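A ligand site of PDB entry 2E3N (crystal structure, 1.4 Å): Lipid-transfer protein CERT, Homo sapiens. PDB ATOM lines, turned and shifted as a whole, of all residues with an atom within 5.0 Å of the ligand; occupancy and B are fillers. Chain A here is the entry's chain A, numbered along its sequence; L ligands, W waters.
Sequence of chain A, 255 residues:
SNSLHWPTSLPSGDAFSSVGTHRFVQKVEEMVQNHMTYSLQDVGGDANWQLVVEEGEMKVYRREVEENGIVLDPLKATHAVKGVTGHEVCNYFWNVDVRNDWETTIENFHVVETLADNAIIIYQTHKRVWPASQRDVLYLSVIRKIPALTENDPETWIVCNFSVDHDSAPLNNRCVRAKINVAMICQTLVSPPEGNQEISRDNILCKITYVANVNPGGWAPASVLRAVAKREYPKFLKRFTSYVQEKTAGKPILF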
ATOM      1  N   PHE A  93      -1.207 -17.633  20.797  1.00  0.00           N
ATOM      2  CA  PHE A  93      -2.112 -17.265  19.697  1.00  0.00           C
ATOM      3  C   PHE A  93      -2.294 -15.747  19.640  1.00  0.00           C
ATOM      4  O   PHE A  93      -2.367 -15.150  18.563  1.00  0.00           O
ATOM      5  CB  PHE A  93      -3.464 -17.956  19.905  1.00  0.00           C
ATOM      6  CG  PHE A  93      -4.414 -17.785  18.748  1.00  0.00           C
ATOM      7  CD1 PHE A  93      -4.078 -18.259  17.469  1.00  0.00           C
ATOM      8  CD2 PHE A  93      -5.643 -17.175  18.927  1.00  0.00           C
ATOM      9  CE1 PHE A  93      -4.948 -18.100  16.397  1.00  0.00           C
ATOM     10  CE2 PHE A  93      -6.531 -17.023  17.855  1.00  0.00           C
ATOM     11  CZ  PHE A  93      -6.187 -17.491  16.596  1.00  0.00           C
ATOM     12  N   ARG A  99       3.874 -13.881  16.279  1.00  0.00           N
ATOM     13  CA  ARG A  99       2.951 -14.153  15.189  1.00  0.00           C
ATOM     14  C   ARG A  99       3.634 -14.699  13.932  1.00  0.00           C
ATOM     15  O   ARG A  99       3.212 -15.700  13.377  1.00  0.00           O
ATOM     16  CB  ARG A  99       2.155 -12.884  14.847  1.00  0.00           C
ATOM     17  CG  ARG A  99       1.093 -13.067  13.770  1.00  0.00           C
ATOM     18  CD  ARG A  99      -0.081 -13.972  14.204  1.00  0.00           C
ATOM     19  NE  ARG A  99      -0.560 -13.714  15.555  1.00  0.00           N
ATOM     20  CZ  ARG A  99      -1.474 -12.801  15.899  1.00  0.00           C
ATOM     21  NH1 ARG A  99      -2.024 -12.004  14.990  1.00  0.00           N
ATOM     22  NH2 ARG A  99      -1.837 -12.683  17.161  1.00  0.00           N
ATOM     23  N   TRP A 102       4.685 -18.505  13.405  1.00  0.00           N
ATOM     24  CA  TRP A 102       3.739 -19.583  13.082  1.00  0.00           C
ATOM     25  C   TRP A 102       2.738 -19.274  11.966  1.00  0.00           C
ATOM     26  O   TRP A 102       2.338 -20.192  11.250  1.00  0.00           O
ATOM     27  CB  TRP A 102       3.017 -20.108  14.331  1.00  0.00           C
ATOM     28  CG  TRP A 102       2.158 -19.100  15.049  1.00  0.00           C
ATOM     29  CD1 TRP A 102       2.504 -18.342  16.146  1.00  0.00           C
ATOM     30  CD2 TRP A 102       0.808 -18.724  14.728  1.00  0.00           C
ATOM     31  NE1 TRP A 102       1.461 -17.539  16.519  1.00  0.00           N
ATOM     32  CE2 TRP A 102       0.408 -17.740  15.667  1.00  0.00           C
ATOM     33  CE3 TRP A 102      -0.100 -19.117  13.734  1.00  0.00           C
ATOM     34  CZ2 TRP A 102      -0.858 -17.150  15.645  1.00  0.00           C
ATOM     35  CZ3 TRP A 102      -1.360 -18.515  13.711  1.00  0.00           C
ATOM     36  CH2 TRP A 102      -1.722 -17.548  14.654  1.00  0.00           C
ATOM     37  N   GLU A 103       2.322 -18.017  11.831  1.00  0.00           N
ATOM     38  CA  GLU A 103       1.299 -17.645  10.837  1.00  0.00           C
ATOM     39  C   GLU A 103       1.928 -17.648   9.449  1.00  0.00           C
ATOM     40  O   GLU A 103       3.018 -17.083   9.268  1.00  0.00           O
ATOM     41  CB  GLU A 103       0.679 -16.287  11.197  1.00  0.00           C
ATOM     42  CG  GLU A 103      -0.320 -15.693  10.186  1.00  0.00           C
ATOM     43  CD  GLU A 103      -1.595 -16.515  10.030  1.00  0.00           C
ATOM     44  OE1 GLU A 103      -2.528 -16.339  10.849  1.00  0.00           O
ATOM     45  OE2 GLU A 103      -1.679 -17.316   9.079  1.00  0.00           O
ATOM     46  N   THR A 105      -0.284 -17.314   6.458  1.00  0.00           N
ATOM     47  CA  THR A 105      -1.258 -16.815   5.471  1.00  0.00           C
ATOM     48  C   THR A 105      -1.268 -15.303   5.299  1.00  0.00           C
ATOM     49  O   THR A 105      -2.060 -14.773   4.516  1.00  0.00           O
ATOM     50  CB  THR A 105      -2.710 -17.292   5.789  1.00  0.00           C
ATOM     51  OG1 THR A 105      -3.196 -16.589   6.952  1.00  0.00           O
ATOM     52  CG2 THR A 105      -2.765 -18.802   5.998  1.00  0.00           C
ATOM     53  N   ILE A 106      -0.430 -14.584   6.037  1.00  0.00           N
ATOM     54  CA  ILE A 106      -0.408 -13.128   5.924  1.00  0.00           C
ATOM     55  C   ILE A 106       0.776 -12.601   5.146  1.00  0.00           C
ATOM     56  O   ILE A 106       1.856 -13.209   5.143  1.00  0.00           O
ATOM     57  CB  ILE A 106      -0.462 -12.406   7.293  1.00  0.00           C
ATOM     58  CG1 ILE A 106       0.758 -12.766   8.152  1.00  0.00           C
ATOM     59  CG2 ILE A 106      -1.782 -12.683   7.994  1.00  0.00           C
ATOM     60  CD1 ILE A 106       0.963 -11.884   9.359  1.00  0.00           C
ATOM     61  N   GLN A 124      -4.259  -6.443   8.946  1.00  0.00           N
ATOM     62  CA  GLN A 124      -3.396  -7.347   8.186  1.00  0.00           C
ATOM     63  C   GLN A 124      -3.884  -7.588   6.775  1.00  0.00           C
ATOM     64  O   GLN A 124      -5.066  -7.460   6.462  1.00  0.00           O
ATOM     65  CB  GLN A 124      -3.124  -8.659   8.927  1.00  0.00           C
ATOM     66  CG  GLN A 124      -4.245  -9.661   8.920  1.00  0.00           C
ATOM     67  CD  GLN A 124      -4.154 -10.650  10.068  1.00  0.00           C
ATOM     68  OE1 GLN A 124      -3.592 -10.356  11.121  1.00  0.00           O
ATOM     69  NE2 GLN A 124      -4.720 -11.828   9.862  1.00  0.00           N
ATOM     70  N   HIS A 126      -3.789 -10.554   3.735  1.00  0.00           N
ATOM     71  CA  HIS A 126      -3.544 -11.960   3.498  1.00  0.00           C
ATOM     72  C   HIS A 126      -2.901 -12.201   2.151  1.00  0.00           C
ATOM     73  O   HIS A 126      -3.103 -11.426   1.228  1.00  0.00           O
ATOM     74  CB  HIS A 126      -4.822 -12.764   3.713  1.00  0.00           C
ATOM     75  CG  HIS A 126      -5.139 -12.938   5.155  1.00  0.00           C
ATOM     76  ND1 HIS A 126      -4.628 -13.977   5.901  1.00  0.00           N
ATOM     77  CD2 HIS A 126      -5.812 -12.142   6.018  1.00  0.00           C
ATOM     78  CE1 HIS A 126      -5.020 -13.838   7.160  1.00  0.00           C
ATOM     79  NE2 HIS A 126      -5.739 -12.737   7.256  1.00  0.00           N
ATOM     80  N   VAL A 129      -4.591 -15.301  -3.220  1.00  0.00           N
ATOM     81  CA  VAL A 129      -4.782 -16.609  -3.818  1.00  0.00           C
ATOM     82  C   VAL A 129      -5.416 -16.402  -5.180  1.00  0.00           C
ATOM     83  O   VAL A 129      -6.563 -15.962  -5.279  1.00  0.00           O
ATOM     84  CB  VAL A 129      -5.666 -17.537  -2.937  1.00  0.00           C
ATOM     85  CG1 VAL A 129      -5.941 -18.850  -3.659  1.00  0.00           C
ATOM     86  CG2 VAL A 129      -4.979 -17.802  -1.597  1.00  0.00           C
ATOM     87  N   ALA A 132      -8.376 -14.721  -7.179  1.00  0.00           N
ATOM     88  CA  ALA A 132      -9.105 -13.748  -6.362  1.00  0.00           C
ATOM     89  C   ALA A 132      -8.267 -12.524  -6.011  1.00  0.00           C
ATOM     90  O   ALA A 132      -7.039 -12.607  -5.883  1.00  0.00           O
ATOM     91  CB  ALA A 132      -9.603 -14.413  -5.096  1.00  0.00           C
ATOM     92  N   ARG A 135      -7.271  -9.952  -0.024  1.00  0.00           N
ATOM     93  CA  ARG A 135      -8.091  -9.498   1.098  1.00  0.00           C
ATOM     94  C   ARG A 135      -7.260  -8.838   2.196  1.00  0.00           C
ATOM     95  O   ARG A 135      -6.122  -9.249   2.452  1.00  0.00           O
ATOM     96  CB  ARG A 135      -8.894 -10.652   1.687  1.00  0.00           C
ATOM     97  CG  ARG A 135     -10.308 -10.795   1.137  1.00  0.00           C
ATOM     98  CD  ARG A 135     -10.333 -11.193  -0.326  1.00  0.00           C
ATOM     99  NE  ARG A 135     -11.711 -11.370  -0.750  1.00  0.00           N
ATOM    100  CZ  ARG A 135     -12.105 -11.575  -2.000  1.00  0.00           C
ATOM    101  NH1 ARG A 135     -11.212 -11.647  -2.975  1.00  0.00           N
ATOM    102  NH2 ARG A 135     -13.393 -11.706  -2.264  1.00  0.00           N
ATOM    103  N   VAL A 137      -7.946  -7.293   6.432  1.00  0.00           N
ATOM    104  CA  VAL A 137      -8.844  -7.491   7.563  1.00  0.00           C
ATOM    105  C   VAL A 137      -8.410  -6.566   8.693  1.00  0.00           C
ATOM    106  O   VAL A 137      -7.203  -6.278   8.834  1.00  0.00           O
ATOM    107  CB  VAL A 137      -8.943  -8.991   7.951  1.00  0.00           C
ATOM    108  CG1 VAL A 137      -7.602  -9.545   8.334  1.00  0.00           C
ATOM    109  CG2 VAL A 137      -9.986  -9.230   9.031  1.00  0.00           C
ATOM    110  N   TYR A 139      -9.251  -6.184  12.799  1.00  0.00           N
ATOM    111  CA  TYR A 139      -9.950  -6.886  13.880  1.00  0.00           C
ATOM    112  C   TYR A 139      -9.417  -6.536  15.258  1.00  0.00           C
ATOM    113  O   TYR A 139      -8.242  -6.191  15.430  1.00  0.00           O
ATOM    114  CB  TYR A 139      -9.909  -8.405  13.691  1.00  0.00           C
ATOM    115  CG  TYR A 139      -8.535  -9.028  13.650  1.00  0.00           C
ATOM    116  CD1 TYR A 139      -8.022  -9.691  14.762  1.00  0.00           C
ATOM    117  CD2 TYR A 139      -7.757  -8.997  12.486  1.00  0.00           C
ATOM    118  CE1 TYR A 139      -6.783 -10.296  14.745  1.00  0.00           C
ATOM    119  CE2 TYR A 139      -6.499  -9.597  12.458  1.00  0.00           C
ATOM    120  CZ  TYR A 139      -6.021 -10.250  13.588  1.00  0.00           C
ATOM    121  OH  TYR A 139      -4.785 -10.847  13.559  1.00  0.00           O
ATOM    122  N   ASN A 161     -10.944 -12.968  17.991  1.00  0.00           N
ATOM    123  CA  ASN A 161     -10.538 -12.050  16.932  1.00  0.00           C
ATOM    124  C   ASN A 161     -11.769 -11.688  16.113  1.00  0.00           C
ATOM    125  O   ASN A 161     -12.324 -12.564  15.426  1.00  0.00           O
ATOM    126  CB  ASN A 161      -9.529 -12.719  15.996  1.00  0.00           C
ATOM    127  CG  ASN A 161      -8.195 -12.988  16.666  1.00  0.00           C
ATOM    128  OD1 ASN A 161      -7.376 -13.768  16.140  1.00  0.00           O
ATOM    129  ND2 ASN A 161      -7.946 -12.339  17.783  1.00  0.00           N
ATOM    130  N   ALA A 178     -12.261  -8.201   4.094  1.00  0.00           N
ATOM    131  CA  ALA A 178     -12.941  -9.340   4.696  1.00  0.00           C
ATOM    132  C   ALA A 178     -13.419  -8.968   6.084  1.00  0.00           C
ATOM    133  O   ALA A 178     -12.918  -8.008   6.677  1.00  0.00           O
ATOM    134  CB  ALA A 178     -12.003 -10.539   4.783  1.00  0.00           C
ATOM    135  N   ILE A 180     -14.280 -10.946   9.852  1.00  0.00           N
ATOM    136  CA  ILE A 180     -14.050 -12.205  10.544  1.00  0.00           C
ATOM    137  C   ILE A 180     -14.636 -12.259  11.951  1.00  0.00           C
ATOM    138  O   ILE A 180     -14.785 -11.240  12.623  1.00  0.00           O
ATOM    139  CB  ILE A 180     -12.541 -12.560  10.596  1.00  0.00           C
ATOM    140  CG1 ILE A 180     -11.781 -11.654  11.569  1.00  0.00           C
ATOM    141  CG2 ILE A 180     -11.939 -12.490   9.188  1.00  0.00           C
ATOM    142  CD1 ILE A 180     -10.355 -12.121  11.884  1.00  0.00           C
ATOM    143  N   VAL A 182     -13.521 -15.036  14.816  1.00  0.00           N
ATOM    144  CA  VAL A 182     -12.689 -16.203  15.096  1.00  0.00           C
ATOM    145  C   VAL A 182     -12.519 -16.337  16.603  1.00  0.00           C
ATOM    146  O   VAL A 182     -12.409 -15.323  17.316  1.00  0.00           O
ATOM    147  CB  VAL A 182     -11.301 -16.050  14.413  1.00  0.00           C
ATOM    148  CG1 VAL A 182     -10.309 -17.095  14.906  1.00  0.00           C
ATOM    149  CG2 VAL A 182     -11.432 -16.108  12.893  1.00  0.00           C
ATOM    150  N   TYR A 210     -11.540 -24.395  18.033  1.00  0.00           N
ATOM    151  CA  TYR A 210     -11.229 -23.246  17.183  1.00  0.00           C
ATOM    152  C   TYR A 210     -12.402 -23.044  16.225  1.00  0.00           C
ATOM    153  O   TYR A 210     -12.806 -23.982  15.532  1.00  0.00           O
ATOM    154  CB  TYR A 210      -9.937 -23.498  16.396  1.00  0.00           C
ATOM    155  CG  TYR A 210      -9.621 -22.424  15.385  1.00  0.00           C
ATOM    156  CD1 TYR A 210      -8.900 -21.285  15.752  1.00  0.00           C
ATOM    157  CD2 TYR A 210     -10.018 -22.566  14.056  1.00  0.00           C
ATOM    158  CE1 TYR A 210      -8.615 -20.297  14.821  1.00  0.00           C
ATOM    159  CE2 TYR A 210      -9.733 -21.578  13.125  1.00  0.00           C
ATOM    160  CZ  TYR A 210      -9.028 -20.453  13.504  1.00  0.00           C
ATOM    161  OH  TYR A 210      -8.736 -19.483  12.585  1.00  0.00           O
ATOM    162  N   VAL A 214     -15.748 -16.521   8.423  1.00  0.00           N
ATOM    163  CA  VAL A 214     -15.115 -15.520   7.575  1.00  0.00           C
ATOM    164  C   VAL A 214     -16.055 -15.115   6.449  1.00  0.00           C
ATOM    165  O   VAL A 214     -16.556 -15.966   5.710  1.00  0.00           O
ATOM    166  CB  VAL A 214     -13.792 -16.049   6.955  1.00  0.00           C
ATOM    167  CG1 VAL A 214     -13.183 -15.043   5.984  1.00  0.00           C
ATOM    168  CG2 VAL A 214     -12.771 -16.385   8.055  1.00  0.00           C
ATOM    169  N   PRO A 216     -15.640 -13.277   3.105  1.00  0.00           N
ATOM    170  CA  PRO A 216     -14.548 -12.819   2.231  1.00  0.00           C
ATOM    171  C   PRO A 216     -14.729 -11.402   1.682  1.00  0.00           C
ATOM    172  O   PRO A 216     -13.815 -10.893   1.037  1.00  0.00           O
ATOM    173  CB  PRO A 216     -14.554 -13.834   1.078  1.00  0.00           C
ATOM    174  CG  PRO A 216     -15.316 -14.987   1.568  1.00  0.00           C
ATOM    175  CD  PRO A 216     -16.311 -14.467   2.554  1.00  0.00           C
ATOM    176  N   ALA A 220     -15.666 -14.773  -4.625  1.00  0.00           N
ATOM    177  CA  ALA A 220     -14.484 -15.599  -4.839  1.00  0.00           C
ATOM    178  C   ALA A 220     -14.945 -16.872  -5.542  1.00  0.00           C
ATOM    179  O   ALA A 220     -16.101 -17.261  -5.386  1.00  0.00           O
ATOM    180  CB  ALA A 220     -13.826 -15.929  -3.501  1.00  0.00           C
ATOM    181  N   PRO A 221     -14.064 -17.536  -6.323  1.00  0.00           N
ATOM    182  CA  PRO A 221     -14.482 -18.806  -6.894  1.00  0.00           C
ATOM    183  C   PRO A 221     -14.640 -19.816  -5.774  1.00  0.00           C
ATOM    184  O   PRO A 221     -13.667 -20.117  -5.063  1.00  0.00           O
ATOM    185  CB  PRO A 221     -13.325 -19.213  -7.807  1.00  0.00           C
ATOM    186  CG  PRO A 221     -12.442 -18.034  -7.903  1.00  0.00           C
ATOM    187  CD  PRO A 221     -12.685 -17.182  -6.709  1.00  0.00           C
ATOM    188  N   VAL A 224     -12.293 -22.951  -5.358  1.00  0.00           N
ATOM    189  CA  VAL A 224     -10.924 -22.524  -5.048  1.00  0.00           C
ATOM    190  C   VAL A 224     -10.843 -22.104  -3.575  1.00  0.00           C
ATOM    191  O   VAL A 224      -9.964 -22.554  -2.839  1.00  0.00           O
ATOM    192  CB  VAL A 224     -10.438 -21.388  -5.990  1.00  0.00           C
ATOM    193  CG1 VAL A 224      -9.024 -20.935  -5.610  1.00  0.00           C
ATOM    194  CG2 VAL A 224     -10.486 -21.839  -7.458  1.00  0.00           C
ATOM    195  N   LEU A 225     -11.779 -21.271  -3.131  1.00  0.00           N
ATOM    196  CA  LEU A 225     -11.822 -20.833  -1.735  1.00  0.00           C
ATOM    197  C   LEU A 225     -11.922 -22.031  -0.801  1.00  0.00           C
ATOM    198  O   LEU A 225     -11.191 -22.135   0.189  1.00  0.00           O
ATOM    199  CB  LEU A 225     -12.996 -19.884  -1.517  1.00  0.00           C
ATOM    200  CG  LEU A 225     -13.176 -19.281  -0.117  1.00  0.00           C
ATOM    201  CD1 LEU A 225     -13.975 -17.998  -0.209  1.00  0.00           C
ATOM    202  CD2 LEU A 225     -13.849 -20.258   0.849  1.00  0.00           C
ATOM    203  N   VAL A 228      -8.642 -24.042  -0.623  1.00  0.00           N
ATOM    204  CA  VAL A 228      -7.677 -23.318   0.199  1.00  0.00           C
ATOM    205  C   VAL A 228      -7.991 -23.497   1.673  1.00  0.00           C
ATOM    206  O   VAL A 228      -7.097 -23.816   2.463  1.00  0.00           O
ATOM    207  CB  VAL A 228      -7.634 -21.810  -0.141  1.00  0.00           C
ATOM    208  CG1 VAL A 228      -6.827 -21.029   0.890  1.00  0.00           C
ATOM    209  CG2 VAL A 228      -7.067 -21.590  -1.539  1.00  0.00           C
ATOM    210  N   GLU A 232      -5.526 -25.062   4.355  1.00  0.00           N
ATOM    211  CA  GLU A 232      -4.844 -24.124   5.231  1.00  0.00           C
ATOM    212  C   GLU A 232      -5.239 -24.172   6.704  1.00  0.00           C
ATOM    213  O   GLU A 232      -4.387 -23.946   7.576  1.00  0.00           O
ATOM    214  CB  GLU A 232      -4.953 -22.699   4.703  1.00  0.00           C
ATOM    215  CG  GLU A 232      -4.258 -22.476   3.370  1.00  0.00           C
ATOM    216  CD  GLU A 232      -2.746 -22.668   3.421  1.00  0.00           C
ATOM    217  OE1 GLU A 232      -2.117 -22.382   4.468  1.00  0.00           O
ATOM    218  OE2 GLU A 232      -2.183 -23.086   2.396  1.00  0.00           O
ATOM    219  N   TYR A 233      -6.492 -24.467   7.017  1.00  0.00           N
ATOM    220  CA  TYR A 233      -6.890 -24.538   8.413  1.00  0.00           C
ATOM    221  C   TYR A 233      -6.210 -25.688   9.149  1.00  0.00           C
ATOM    222  O   TYR A 233      -5.646 -25.457  10.210  1.00  0.00           O
ATOM    223  CB  TYR A 233      -8.419 -24.557   8.589  1.00  0.00           C
ATOM    224  CG  TYR A 233      -9.054 -23.199   8.454  1.00  0.00           C
ATOM    225  CD1 TYR A 233      -9.776 -22.864   7.315  1.00  0.00           C
ATOM    226  CD2 TYR A 233      -8.928 -22.253   9.479  1.00  0.00           C
ATOM    227  CE1 TYR A 233     -10.370 -21.617   7.195  1.00  0.00           C
ATOM    228  CE2 TYR A 233      -9.522 -21.005   9.369  1.00  0.00           C
ATOM    229  CZ  TYR A 233     -10.246 -20.694   8.223  1.00  0.00           C
ATOM    230  OH  TYR A 233     -10.842 -19.470   8.095  1.00  0.00           O
ATOM    231  N   PHE A 236      -2.548 -24.792   9.609  1.00  0.00           N
ATOM    232  CA  PHE A 236      -2.402 -23.840  10.704  1.00  0.00           C
ATOM    233  C   PHE A 236      -2.497 -24.524  12.068  1.00  0.00           C
ATOM    234  O   PHE A 236      -1.647 -24.320  12.942  1.00  0.00           O
ATOM    235  CB  PHE A 236      -3.441 -22.716  10.583  1.00  0.00           C
ATOM    236  CG  PHE A 236      -3.990 -22.241  11.904  1.00  0.00           C
ATOM    237  CD1 PHE A 236      -3.197 -21.539  12.793  1.00  0.00           C
ATOM    238  CD2 PHE A 236      -5.312 -22.523  12.263  1.00  0.00           C
ATOM    239  CE1 PHE A 236      -3.704 -21.123  14.033  1.00  0.00           C
ATOM    240  CE2 PHE A 236      -5.818 -22.108  13.492  1.00  0.00           C
ATOM    241  CZ  PHE A 236      -5.015 -21.404  14.372  1.00  0.00           C
HETATM  242  O1  LIG L   1      -6.911 -17.579  13.230  1.00  0.00           O
HETATM  243  C1  LIG L   1      -5.855 -17.562  12.613  1.00  0.00           C
HETATM  244  N1  LIG L   1      -5.002 -16.530  12.626  1.00  0.00           N
HETATM  245  C2  LIG L   1      -5.265 -15.235  13.269  1.00  0.00           C
HETATM  246  C3  LIG L   1      -3.979 -14.392  13.241  1.00  0.00           C
HETATM  247  O2  LIG L   1      -3.608 -14.045  11.890  1.00  0.00           O
HETATM  248  C4  LIG L   1      -6.502 -14.507  12.696  1.00  0.00           C
HETATM  249  C5  LIG L   1      -6.642 -14.770  11.201  1.00  0.00           C
HETATM  250  C6  LIG L   1      -7.787 -15.149  10.630  1.00  0.00           C
HETATM  251  C7  LIG L   1      -7.832 -15.408   9.138  1.00  0.00           C
HETATM  252  C8  LIG L   1      -8.606 -14.351   8.380  1.00  0.00           C
HETATM  253  C9  LIG L   1      -8.668 -14.681   6.886  1.00  0.00           C
HETATM  254  C10 LIG L   1      -9.339 -13.530   6.140  1.00  0.00           C
HETATM  255  C11 LIG L   1      -8.968 -13.501   4.668  1.00  0.00           C
HETATM  256  C12 LIG L   1     -10.171 -13.987   3.876  1.00  0.00           C
HETATM  257  C13 LIG L   1      -9.780 -14.355   2.445  1.00  0.00           C
HETATM  258  C14 LIG L   1     -10.933 -15.086   1.767  1.00  0.00           C
HETATM  259  C15 LIG L   1     -10.931 -14.900   0.251  1.00  0.00           C
HETATM  260  C16 LIG L   1      -9.833 -15.715  -0.421  1.00  0.00           C
HETATM  261  C17 LIG L   1     -10.316 -16.257  -1.763  1.00  0.00           C
HETATM  262  C18 LIG L   1      -9.434 -17.403  -2.230  1.00  0.00           C
HETATM  263  C19 LIG L   1      -9.805 -17.815  -3.634  1.00  0.00           C
HETATM  264  O3  LIG L   1      -7.678 -14.942  13.422  1.00  0.00           O
HETATM  265  C20 LIG L   1      -5.441 -18.723  11.757  1.00  0.00           C
HETATM  266  C21 LIG L   1      -6.078 -18.508  10.384  1.00  0.00           C
HETATM  267  C22 LIG L   1      -5.838 -19.689   9.463  1.00  0.00           C
HETATM  268  C23 LIG L   1      -6.348 -19.389   8.054  1.00  0.00           C
HETATM  269  C24 LIG L   1      -6.189 -20.637   7.179  1.00  0.00           C
HETATM  270  O   HOH W   1      -1.569 -12.036  12.096  1.00  0.00           O
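Residues that only touch the ligand: Phe 93 (3.4 Å), Arg 99 (3.5 Å), Trp 102 (3.99 Å), His 126 (3.5 Å), Val 129 (3.8 Å), Ala 132 (3.7 Å), Arg 135 (3.8 Å), Tyr 139 (3.6 Å), Ile 180 (3.9 Å), Val 182 (3.7 Å), Val 214 (3.8 Å), Pro 216 (3.9 Å), Ala 220 (3.9 Å), Val 224 (3.8 Å), Glu 232 (3.5 Å), Tyr 233 (3.8 Å) and Phe 236 (3.7 Å). Hydrophobic or aromatic side chains that line the ligand: Phe 93, Trp 102, His 126, Val 129, Ala 132, Ile 180, Val 182, Tyr 210, Val 214, Pro 216, Ala 220, Val 224, Tyr 233 and Phe 236. Within 4 Å of the ligand: Phe 93, Arg 99, Trp 102, Glu 103, Gln 124, His 126, Val 129, Ala 132, Arg 135, Tyr 139, Asn 161, Ile 180, Val 182, Tyr 210, Val 214, Pro 216, Ala 220, Val 224, Glu 232, Tyr 233 and Phe 236.
OE2 of Glu 103 lies within hydrogen-bond range of OG1 of Thr 105, at 2.7 Å. O of Asn 161 sits at hydrogen-bond distance from N of Val 182. The side-chain amide nitrogen (NE2) of Gln 124 is in hydrogen-bond range of a ring nitrogen (NE2) of His 126, at 2.9 Å. OE1 of Gln 124 sits at hydrogen-bond distance from OH of Tyr 139 (2.8 Å). N of Val 137 sits at hydrogen-bond distance from O of Gln 124 (2.9 Å). The backbone carbonyl oxygen (O) of Arg 135 sits at hydrogen-bond distance from the backbone NH (N) of His 126 (3.0 Å). O of Thr 105 is in hydrogen-bond range of ND1 of His 126 (3.0 Å). NH1 of Arg 99 sits at hydrogen-bond distance from OH of Tyr 139, 3.3 Å away.
OH of Tyr 210 lies within hydrogen-bond range of O1 of the ligand (2.7 Å). OE1 of Glu 103 is in hydrogen-bond range of O2 of the ligand (2.7 Å). The side-chain amide oxygen (OD1) of Asn 161 is in hydrogen-bond range of an oxygen (O3) of the ligand (3.0 Å). The side-chain amide nitrogen (NE2) of Gln 124 is in hydrogen-bond range of an oxygen (O2) of the ligand (3.2 Å).
Water W1 lies within hydrogen-bond range of the side-chain amide oxygen (OE1) of Gln 124 (2.8 Å), an oxygen (O2) of the ligand (2.9 Å) and the guanidinium group (NH1) of Arg 99 (2.9 Å).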
